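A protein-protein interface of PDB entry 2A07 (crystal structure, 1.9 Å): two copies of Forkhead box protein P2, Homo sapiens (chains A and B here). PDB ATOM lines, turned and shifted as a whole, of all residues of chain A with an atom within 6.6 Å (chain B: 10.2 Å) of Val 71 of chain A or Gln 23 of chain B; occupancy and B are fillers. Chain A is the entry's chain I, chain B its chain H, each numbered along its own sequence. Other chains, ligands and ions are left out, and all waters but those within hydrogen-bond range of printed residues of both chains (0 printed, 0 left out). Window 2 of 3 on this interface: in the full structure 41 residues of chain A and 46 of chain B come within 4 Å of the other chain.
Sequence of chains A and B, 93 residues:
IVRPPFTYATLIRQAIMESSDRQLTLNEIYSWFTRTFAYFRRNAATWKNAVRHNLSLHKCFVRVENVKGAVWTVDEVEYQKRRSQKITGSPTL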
ATOM      1  N   VAL A  62       9.315  27.979  24.634  1.00  0.00           N
ATOM      2  CA  VAL A  62       9.615  27.146  23.469  1.00  0.00           C
ATOM      3  C   VAL A  62       8.591  26.026  23.308  1.00  0.00           C
ATOM      4  O   VAL A  62       8.297  25.300  24.256  1.00  0.00           O
ATOM      5  CB  VAL A  62      11.011  26.500  23.586  1.00  0.00           C
ATOM      6  CG1 VAL A  62      11.363  25.796  22.285  1.00  0.00           C
ATOM      7  CG2 VAL A  62      12.043  27.561  23.920  1.00  0.00           C
ATOM      8  N   ARG A  63       8.064  25.878  22.098  1.00  0.00           N
ATOM      9  CA  ARG A  63       7.083  24.840  21.822  1.00  0.00           C
ATOM     10  C   ARG A  63       7.752  23.533  21.388  1.00  0.00           C
ATOM     11  O   ARG A  63       8.364  23.451  20.320  1.00  0.00           O
ATOM     12  CB  ARG A  63       6.088  25.311  20.751  1.00  0.00           C
ATOM     13  CG  ARG A  63       6.698  25.758  19.429  1.00  0.00           C
ATOM     14  CD  ARG A  63       5.636  26.438  18.570  1.00  0.00           C
ATOM     15  NE  ARG A  63       6.141  26.928  17.289  1.00  0.00           N
ATOM     16  CZ  ARG A  63       5.413  27.649  16.440  1.00  0.00           C
ATOM     17  NH1 ARG A  63       4.156  27.960  16.740  1.00  0.00           N
ATOM     18  NH2 ARG A  63       5.931  28.057  15.289  1.00  0.00           N
ATOM     19  N   VAL A  64       7.643  22.517  22.240  1.00  0.00           N
ATOM     20  CA  VAL A  64       8.225  21.201  21.976  1.00  0.00           C
ATOM     21  C   VAL A  64       7.161  20.245  21.445  1.00  0.00           C
ATOM     22  O   VAL A  64       6.232  19.874  22.160  1.00  0.00           O
ATOM     23  CB  VAL A  64       8.853  20.590  23.266  1.00  0.00           C
ATOM     24  CG1 VAL A  64       9.442  19.240  22.970  1.00  0.00           C
ATOM     25  CG2 VAL A  64       9.892  21.532  23.827  1.00  0.00           C
ATOM     26  N   GLU A  65       7.321  19.836  20.191  1.00  0.00           N
ATOM     27  CA  GLU A  65       6.381  18.927  19.556  1.00  0.00           C
ATOM     28  C   GLU A  65       6.731  17.471  19.850  1.00  0.00           C
ATOM     29  O   GLU A  65       7.725  16.945  19.347  1.00  0.00           O
ATOM     30  CB  GLU A  65       6.360  19.173  18.046  1.00  0.00           C
ATOM     31  CG  GLU A  65       5.902  20.578  17.656  1.00  0.00           C
ATOM     32  CD  GLU A  65       5.917  20.801  16.157  1.00  0.00           C
ATOM     33  OE1 GLU A  65       7.000  20.659  15.550  1.00  0.00           O
ATOM     34  OE2 GLU A  65       4.848  21.116  15.589  1.00  0.00           O
ATOM     35  N   ASN A  66       5.903  16.829  20.672  1.00  0.00           N
ATOM     36  CA  ASN A  66       6.114  15.436  21.046  1.00  0.00           C
ATOM     37  C   ASN A  66       5.067  14.530  20.411  1.00  0.00           C
ATOM     38  O   ASN A  66       4.335  14.945  19.512  1.00  0.00           O
ATOM     39  CB  ASN A  66       6.061  15.282  22.569  1.00  0.00           C
ATOM     40  CG  ASN A  66       4.708  15.670  23.152  1.00  0.00           C
ATOM     41  OD1 ASN A  66       4.461  15.492  24.345  1.00  0.00           O
ATOM     42  ND2 ASN A  66       3.828  16.207  22.312  1.00  0.00           N
ATOM     43  N   LYS A  68       2.159  13.790  20.725  1.00  0.00           N
ATOM     44  CA  LYS A  68       0.838  14.193  21.201  1.00  0.00           C
ATOM     45  C   LYS A  68       0.273  15.324  20.346  1.00  0.00           C
ATOM     46  O   LYS A  68      -0.938  15.409  20.135  1.00  0.00           O
ATOM     47  CB  LYS A  68       0.911  14.640  22.665  1.00  0.00           C
ATOM     48  CG  LYS A  68       1.228  13.514  23.640  1.00  0.00           C
ATOM     49  CD  LYS A  68       1.294  14.002  25.078  1.00  0.00           C
ATOM     50  CE  LYS A  68       1.605  12.855  26.028  1.00  0.00           C
ATOM     51  NZ  LYS A  68       1.665  13.300  27.449  1.00  0.00           N
ATOM     52  N   GLY A  69       1.157  16.188  19.857  1.00  0.00           N
ATOM     53  CA  GLY A  69       0.724  17.299  19.030  1.00  0.00           C
ATOM     54  C   GLY A  69       1.611  18.519  19.192  1.00  0.00           C
ATOM     55  O   GLY A  69       2.359  18.875  18.281  1.00  0.00           O
ATOM     56  N   ALA A  70       1.529  19.160  20.353  1.00  0.00           N
ATOM     57  CA  ALA A  70       2.332  20.346  20.628  1.00  0.00           C
ATOM     58  C   ALA A  70       2.216  20.771  22.086  1.00  0.00           C
ATOM     59  O   ALA A  70       1.115  20.926  22.613  1.00  0.00           O
ATOM     60  CB  ALA A  70       1.899  21.489  19.719  1.00  0.00           C
ATOM     61  N   VAL A  71       3.358  20.956  22.735  1.00  0.00           N
ATOM     62  CA  VAL A  71       3.378  21.376  24.128  1.00  0.00           C
ATOM     63  C   VAL A  71       4.377  22.511  24.300  1.00  0.00           C
ATOM     64  O   VAL A  71       5.444  22.507  23.689  1.00  0.00           O
ATOM     65  CB  VAL A  71       3.778  20.217  25.067  1.00  0.00           C
ATOM     66  CG1 VAL A  71       2.870  19.024  24.830  1.00  0.00           C
ATOM     67  CG2 VAL A  71       5.232  19.836  24.848  1.00  0.00           C
ATOM     68  N   TRP A  72       4.025  23.487  25.126  1.00  0.00           N
ATOM     69  CA  TRP A  72       4.915  24.607  25.369  1.00  0.00           C
ATOM     70  C   TRP A  72       5.673  24.386  26.660  1.00  0.00           C
ATOM     71  O   TRP A  72       5.120  23.886  27.638  1.00  0.00           O
ATOM     72  CB  TRP A  72       4.132  25.913  25.454  1.00  0.00           C
ATOM     73  CG  TRP A  72       3.513  26.298  24.163  1.00  0.00           C
ATOM     74  CD1 TRP A  72       2.314  25.874  23.667  1.00  0.00           C
ATOM     75  CD2 TRP A  72       4.069  27.175  23.184  1.00  0.00           C
ATOM     76  NE1 TRP A  72       2.088  26.438  22.435  1.00  0.00           N
ATOM     77  CE2 TRP A  72       3.153  27.239  22.112  1.00  0.00           C
ATOM     78  CE3 TRP A  72       5.261  27.908  23.103  1.00  0.00           C
ATOM     79  CZ2 TRP A  72       3.382  28.018  20.977  1.00  0.00           C
ATOM     80  CZ3 TRP A  72       5.490  28.683  21.975  1.00  0.00           C
ATOM     81  CH2 TRP A  72       4.556  28.728  20.924  1.00  0.00           C
ATOM     82  N   THR A  73       6.946  24.757  26.656  1.00  0.00           N
ATOM     83  CA  THR A  73       7.785  24.597  27.831  1.00  0.00           C
ATOM     84  C   THR A  73       8.459  25.925  28.154  1.00  0.00           C
ATOM     85  O   THR A  73       8.328  26.893  27.405  1.00  0.00           O
ATOM     86  CB  THR A  73       8.856  23.520  27.597  1.00  0.00           C
ATOM     87  OG1 THR A  73       9.595  23.308  28.805  1.00  0.00           O
ATOM     88  CG2 THR A  73       9.807  23.946  26.485  1.00  0.00           C
ATOM     89  N   ILE B  12       2.138  32.618  32.534  1.00  0.00           N
ATOM     90  CA  ILE B  12       2.317  31.475  31.653  1.00  0.00           C
ATOM     91  C   ILE B  12       3.365  30.551  32.263  1.00  0.00           C
ATOM     92  O   ILE B  12       3.237  29.329  32.186  1.00  0.00           O
ATOM     93  CB  ILE B  12       2.795  31.898  30.248  1.00  0.00           C
ATOM     94  CG1 ILE B  12       1.688  32.684  29.536  1.00  0.00           C
ATOM     95  CG2 ILE B  12       3.177  30.659  29.428  1.00  0.00           C
ATOM     96  CD1 ILE B  12       2.109  33.276  28.198  1.00  0.00           C
ATOM     97  N   ARG B  13       4.401  31.134  32.865  1.00  0.00           N
ATOM     98  CA  ARG B  13       5.449  30.327  33.480  1.00  0.00           C
ATOM     99  C   ARG B  13       4.903  29.600  34.699  1.00  0.00           C
ATOM    100  O   ARG B  13       5.184  28.416  34.905  1.00  0.00           O
ATOM    101  CB  ARG B  13       6.644  31.180  33.906  1.00  0.00           C
ATOM    102  CG  ARG B  13       7.652  30.388  34.734  1.00  0.00           C
ATOM    103  CD  ARG B  13       8.850  31.219  35.136  1.00  0.00           C
ATOM    104  NE  ARG B  13       9.735  30.512  36.060  1.00  0.00           N
ATOM    105  CZ  ARG B  13       9.435  30.246  37.328  1.00  0.00           C
ATOM    106  NH1 ARG B  13       8.271  30.628  37.835  1.00  0.00           N
ATOM    107  NH2 ARG B  13      10.303  29.599  38.095  1.00  0.00           N
ATOM    108  N   GLN B  14       4.130  30.311  35.513  1.00  0.00           N
ATOM    109  CA  GLN B  14       3.546  29.708  36.704  1.00  0.00           C
ATOM    110  C   GLN B  14       2.739  28.470  36.329  1.00  0.00           C
ATOM    111  O   GLN B  14       2.864  27.417  36.968  1.00  0.00           O
ATOM    112  CB  GLN B  14       2.639  30.709  37.426  1.00  0.00           C
ATOM    113  CG  GLN B  14       2.282  30.286  38.849  1.00  0.00           C
ATOM    114  CD  GLN B  14       1.282  31.217  39.521  1.00  0.00           C
ATOM    115  OE1 GLN B  14       1.307  32.433  39.313  1.00  0.00           O
ATOM    116  NE2 GLN B  14       0.406  30.646  40.352  1.00  0.00           N
ATOM    117  N   ALA B  15       1.910  28.599  35.298  1.00  0.00           N
ATOM    118  CA  ALA B  15       1.081  27.492  34.833  1.00  0.00           C
ATOM    119  C   ALA B  15       1.943  26.292  34.452  1.00  0.00           C
ATOM    120  O   ALA B  15       1.810  25.206  35.021  1.00  0.00           O
ATOM    121  CB  ALA B  15       0.249  27.933  33.640  1.00  0.00           C
ATOM    122  N   ILE B  16       2.826  26.495  33.479  1.00  0.00           N
ATOM    123  CA  ILE B  16       3.710  25.435  33.022  1.00  0.00           C
ATOM    124  C   ILE B  16       4.536  24.872  34.180  1.00  0.00           C
ATOM    125  O   ILE B  16       4.625  23.658  34.354  1.00  0.00           O
ATOM    126  CB  ILE B  16       4.660  25.953  31.920  1.00  0.00           C
ATOM    127  CG1 ILE B  16       3.846  26.355  30.685  1.00  0.00           C
ATOM    128  CG2 ILE B  16       5.695  24.888  31.576  1.00  0.00           C
ATOM    129  CD1 ILE B  16       4.667  26.989  29.587  1.00  0.00           C
ATOM    130  N   MET B  17       5.122  25.762  34.974  1.00  0.00           N
ATOM    131  CA  MET B  17       5.953  25.363  36.105  1.00  0.00           C
ATOM    132  C   MET B  17       5.198  24.540  37.144  1.00  0.00           C
ATOM    133  O   MET B  17       5.791  23.712  37.839  1.00  0.00           O
ATOM    134  CB  MET B  17       6.554  26.599  36.778  1.00  0.00           C
ATOM    135  CG  MET B  17       7.744  26.292  37.663  1.00  0.00           C
ATOM    136  SD  MET B  17       9.010  25.382  36.739  1.00  0.00           S
ATOM    137  CE  MET B  17       9.999  26.710  36.111  1.00  0.00           C
ATOM    138  N   GLU B  18       3.894  24.774  37.258  1.00  0.00           N
ATOM    139  CA  GLU B  18       3.081  24.047  38.221  1.00  0.00           C
ATOM    140  C   GLU B  18       2.190  23.068  37.476  1.00  0.00           C
ATOM    141  O   GLU B  18       0.970  23.229  37.373  1.00  0.00           O
ATOM    142  CB  GLU B  18       2.255  25.021  39.064  1.00  0.00           C
ATOM    143  CG  GLU B  18       3.128  26.029  39.808  1.00  0.00           C
ATOM    144  CD  GLU B  18       2.326  26.978  40.688  1.00  0.00           C
ATOM    145  OE1 GLU B  18       1.106  27.108  40.460  1.00  0.00           O
ATOM    146  OE2 GLU B  18       2.923  27.599  41.596  1.00  0.00           O
ATOM    147  N   SER B  19       2.853  22.045  36.953  1.00  0.00           N
ATOM    148  CA  SER B  19       2.234  20.971  36.198  1.00  0.00           C
ATOM    149  C   SER B  19       3.338  19.930  36.052  1.00  0.00           C
ATOM    150  O   SER B  19       4.502  20.288  35.837  1.00  0.00           O
ATOM    151  CB  SER B  19       1.817  21.468  34.816  1.00  0.00           C
ATOM    152  OG  SER B  19       2.960  21.733  34.014  1.00  0.00           O
ATOM    153  N   SER B  20       2.976  18.656  36.200  1.00  0.00           N
ATOM    154  CA  SER B  20       3.919  17.546  36.070  1.00  0.00           C
ATOM    155  C   SER B  20       4.289  17.354  34.608  1.00  0.00           C
ATOM    156  O   SER B  20       3.424  17.269  33.741  1.00  0.00           O
ATOM    157  CB  SER B  20       3.322  16.249  36.624  1.00  0.00           C
ATOM    158  OG  SER B  20       4.270  15.195  36.596  1.00  0.00           O
ATOM    159  N   ASP B  21       5.596  17.280  34.378  1.00  0.00           N
ATOM    160  CA  ASP B  21       6.231  17.136  33.067  1.00  0.00           C
ATOM    161  C   ASP B  21       6.614  18.520  32.582  1.00  0.00           C
ATOM    162  O   ASP B  21       7.141  18.674  31.485  1.00  0.00           O
ATOM    163  CB  ASP B  21       5.302  16.490  32.034  1.00  0.00           C
ATOM    164  CG  ASP B  21       4.931  15.066  32.386  1.00  0.00           C
ATOM    165  OD1 ASP B  21       4.235  14.432  31.568  1.00  0.00           O
ATOM    166  OD2 ASP B  21       5.334  14.587  33.468  1.00  0.00           O
ATOM    167  N   ARG B  22       6.314  19.523  33.402  1.00  0.00           N
ATOM    168  CA  ARG B  22       6.605  20.918  33.084  1.00  0.00           C
ATOM    169  C   ARG B  22       6.306  21.285  31.634  1.00  0.00           C
ATOM    170  O   ARG B  22       7.065  22.007  30.988  1.00  0.00           O
ATOM    171  CB  ARG B  22       8.062  21.243  33.413  1.00  0.00           C
ATOM    172  CG  ARG B  22       8.394  21.074  34.888  1.00  0.00           C
ATOM    173  CD  ARG B  22       9.792  21.571  35.191  1.00  0.00           C
ATOM    174  NE  ARG B  22      10.144  21.420  36.598  1.00  0.00           N
ATOM    175  CZ  ARG B  22      11.300  21.818  37.119  1.00  0.00           C
ATOM    176  NH1 ARG B  22      12.211  22.392  36.346  1.00  0.00           N
ATOM    177  NH2 ARG B  22      11.547  21.643  38.411  1.00  0.00           N
ATOM    178  N   GLN B  23       5.188  20.774  31.131  1.00  0.00           N
ATOM    179  CA  GLN B  23       4.755  21.042  29.766  1.00  0.00           C
ATOM    180  C   GLN B  23       3.249  21.252  29.757  1.00  0.00           C
ATOM    181  O   GLN B  23       2.543  20.760  30.635  1.00  0.00           O
ATOM    182  CB  GLN B  23       5.086  19.870  28.843  1.00  0.00           C
ATOM    183  CG  GLN B  23       6.549  19.510  28.761  1.00  0.00           C
ATOM    184  CD  GLN B  23       6.796  18.379  27.786  1.00  0.00           C
ATOM    185  OE1 GLN B  23       6.143  17.338  27.851  1.00  0.00           O
ATOM    186  NE2 GLN B  23       7.744  18.576  26.875  1.00  0.00           N
ATOM    187  N   LEU B  24       2.769  21.984  28.760  1.00  0.00           N
ATOM    188  CA  LEU B  24       1.347  22.253  28.617  1.00  0.00           C
ATOM    189  C   LEU B  24       1.035  22.622  27.179  1.00  0.00           C
ATOM    190  O   LEU B  24       1.781  23.363  26.542  1.00  0.00           O
ATOM    191  CB  LEU B  24       0.909  23.407  29.528  1.00  0.00           C
ATOM    192  CG  LEU B  24       0.934  23.227  31.049  1.00  0.00           C
ATOM    193  CD1 LEU B  24       0.458  24.508  31.718  1.00  0.00           C
ATOM    194  CD2 LEU B  24       0.042  22.062  31.448  1.00  0.00           C
ATOM    195  N   THR B  25      -0.064  22.090  26.662  1.00  0.00           N
ATOM    196  CA  THR B  25      -0.485  22.403  25.305  1.00  0.00           C
ATOM    197  C   THR B  25      -1.142  23.776  25.400  1.00  0.00           C
ATOM    198  O   THR B  25      -1.454  24.234  26.503  1.00  0.00           O
ATOM    199  CB  THR B  25      -1.533  21.398  24.809  1.00  0.00           C
ATOM    200  OG1 THR B  25      -2.708  21.499  25.621  1.00  0.00           O
ATOM    201  CG2 THR B  25      -0.992  19.982  24.893  1.00  0.00           C
ATOM    202  N   LEU B  26      -1.363  24.424  24.263  1.00  0.00           N
ATOM    203  CA  LEU B  26      -1.995  25.735  24.277  1.00  0.00           C
ATOM    204  C   LEU B  26      -3.372  25.650  24.932  1.00  0.00           C
ATOM    205  O   LEU B  26      -3.794  26.571  25.626  1.00  0.00           O
ATOM    206  CB  LEU B  26      -2.141  26.290  22.857  1.00  0.00           C
ATOM    207  CG  LEU B  26      -2.859  27.647  22.790  1.00  0.00           C
ATOM    208  CD1 LEU B  26      -2.080  28.685  23.596  1.00  0.00           C
ATOM    209  CD2 LEU B  26      -3.006  28.093  21.343  1.00  0.00           C
ATOM    210  N   ASN B  27      -4.074  24.543  24.718  1.00  0.00           N
ATOM    211  CA  ASN B  27      -5.397  24.403  25.311  1.00  0.00           C
ATOM    212  C   ASN B  27      -5.321  24.274  26.825  1.00  0.00           C
ATOM    213  O   ASN B  27      -6.186  24.786  27.540  1.00  0.00           O
ATOM    214  CB  ASN B  27      -6.135  23.194  24.739  1.00  0.00           C
ATOM    215  CG  ASN B  27      -7.584  23.145  25.187  1.00  0.00           C
ATOM    216  OD1 ASN B  27      -8.372  24.037  24.870  1.00  0.00           O
ATOM    217  ND2 ASN B  27      -7.939  22.111  25.940  1.00  0.00           N
ATOM    218  N   GLU B  28      -4.290  23.587  27.306  1.00  0.00           N
ATOM    219  CA  GLU B  28      -4.089  23.393  28.739  1.00  0.00           C
ATOM    220  C   GLU B  28      -3.735  24.715  29.417  1.00  0.00           C
ATOM    221  O   GLU B  28      -4.119  24.968  30.566  1.00  0.00           O
ATOM    222  CB  GLU B  28      -2.983  22.365  28.971  1.00  0.00           C
ATOM    223  CG  GLU B  28      -3.393  20.944  28.621  1.00  0.00           C
ATOM    224  CD  GLU B  28      -2.225  19.979  28.640  1.00  0.00           C
ATOM    225  OE1 GLU B  28      -1.210  20.282  29.303  1.00  0.00           O
ATOM    226  OE2 GLU B  28      -2.329  18.911  28.001  1.00  0.00           O
ATOM    227  N   ILE B  29      -2.986  25.556  28.710  1.00  0.00           N
ATOM    228  CA  ILE B  29      -2.630  26.860  29.245  1.00  0.00           C
ATOM    229  C   ILE B  29      -3.921  27.664  29.317  1.00  0.00           C
ATOM    230  O   ILE B  29      -4.175  28.343  30.309  1.00  0.00           O
ATOM    231  CB  ILE B  29      -1.592  27.577  28.347  1.00  0.00           C
ATOM    232  CG1 ILE B  29      -0.240  26.868  28.476  1.00  0.00           C
ATOM    233  CG2 ILE B  29      -1.485  29.050  28.741  1.00  0.00           C
ATOM    234  CD1 ILE B  29       0.823  27.365  27.510  1.00  0.00           C
ATOM    235  N   TRP B  32      -5.868  26.724  32.344  1.00  0.00           N
ATOM    236  CA  TRP B  32      -5.279  27.287  33.554  1.00  0.00           C
ATOM    237  C   TRP B  32      -5.658  28.766  33.684  1.00  0.00           C
ATOM    238  O   TRP B  32      -6.029  29.226  34.766  1.00  0.00           O
ATOM    239  CB  TRP B  32      -3.753  27.127  33.530  1.00  0.00           C
ATOM    240  CG  TRP B  32      -3.083  27.491  34.821  1.00  0.00           C
ATOM    241  CD1 TRP B  32      -2.780  26.653  35.859  1.00  0.00           C
ATOM    242  CD2 TRP B  32      -2.631  28.791  35.212  1.00  0.00           C
ATOM    243  NE1 TRP B  32      -2.161  27.351  36.870  1.00  0.00           N
ATOM    244  CE2 TRP B  32      -2.059  28.667  36.497  1.00  0.00           C
ATOM    245  CE3 TRP B  32      -2.656  30.049  34.599  1.00  0.00           C
ATOM    246  CZ2 TRP B  32      -1.510  29.760  37.183  1.00  0.00           C
ATOM    247  CZ3 TRP B  32      -2.110  31.138  35.282  1.00  0.00           C
ATOM    248  CH2 TRP B  32      -1.544  30.983  36.561  1.00  0.00           C
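O of Leu 24 of chain B sits at hydrogen-bond distance from N of Trp 72 of chain A.
The side-chain hydroxyl (OG1) of Thr 25 of chain B lies within hydrogen-bond range of the backbone NH (N) of Glu 28 of chain B. O of Val 71 of chain A lies within hydrogen-bond range of N of Val 64 of chain A, at 2.6 Å. The backbone carbonyl oxygen (O) of Val 62 of chain A lies within hydrogen-bond range of the backbone NH (N) of Thr 73 of chain A (2.8 Å). The side-chain hydroxyl (OG1) of Thr 25 of chain B sits close to the backbone NH (N) of Asn 27 of chain B (3.5 Å). The backbone carbonyl oxygen (O) of Ile 16 of chain B sits at hydrogen-bond distance from the side-chain hydroxyl (OG) of Ser 19 of chain B (2.6 Å).
Among the printed residues, pairs that only touch across the chains: Ala 70 of chain A with Thr 25 of chain B, Val 71 of chain A with Gln 23 of chain B, Val 71 of chain A with Leu 24 of chain B, Val 71 of chain A with Thr 25 of chain B, Trp 72 of chain A with Ile 16 of chain B, Trp 72 of chain A with Gln 23 of chain B, Trp 72 of chain A with Leu 26 of chain B and Thr 73 of chain A with Arg 22 of chain B.
Printed residues of chain A that touch a printed residue of chain B: Ala 70, Val 71, Trp 72 and Thr 73. Hydrophobic or aromatic side chains of chain A that line the printed part of chain B: Val 71 and Trp 72. Hydrophobic or aromatic side chains of chain B that line the printed part of chain A: Ile 16. Among the printed residues, 9 pairs touch across the chains. Among the printed residues, no Asp or Glu carboxylate lies within 4 Å of a Lys or Arg side-chain nitrogen of the other chain.
No residue of chain B comes within 4 Å of Gly 69 of chain A. Printed residues of chain B within 4 Å of Ala 70 of chain A: Thr 25. Val 71 of chain A touches just these residues of chain B: Gln 23 (3.5 Å), Leu 24 (3.5 Å) and Thr 25 (3.98 Å). Of the printed residues of chain B, Thr 73 of chain A touches Arg 22 (3.6 Å). Glu 18 of chain B touches none of the printed residues of chain A. Ser 20 of chain B touches none of the printed residues of chain A. Of the printed residues of chain A, Arg 22 of chain B touches Thr 73. Of chain A, only Val 71 (3.5 Å) and Trp 72 (3.6 Å) come within 4 Å of Gln 23 of chain B. Of the printed residues of chain A, Leu 24 of chain B touches Val 71 and Trp 72. Of the printed residues of chain A, Thr 25 of chain B touches Ala 70 (3.2 Å) and Val 71 (3.98 Å). Printed residues of chain A within 4 Å of Leu 26 of chain B: Trp 72. The nearest residue of chain B that does not touch Val 71 of chain A is Leu 26 of chain B (5.6 Å). The nearest printed residue of chain A that does not touch Thr 25 of chain B is Trp 72 of chain A (4.4 Å).
No position is printed for both chains. Of the 9 pairs that touch across the chains among the printed residues, none has its exchanged pair printed and touching as well.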
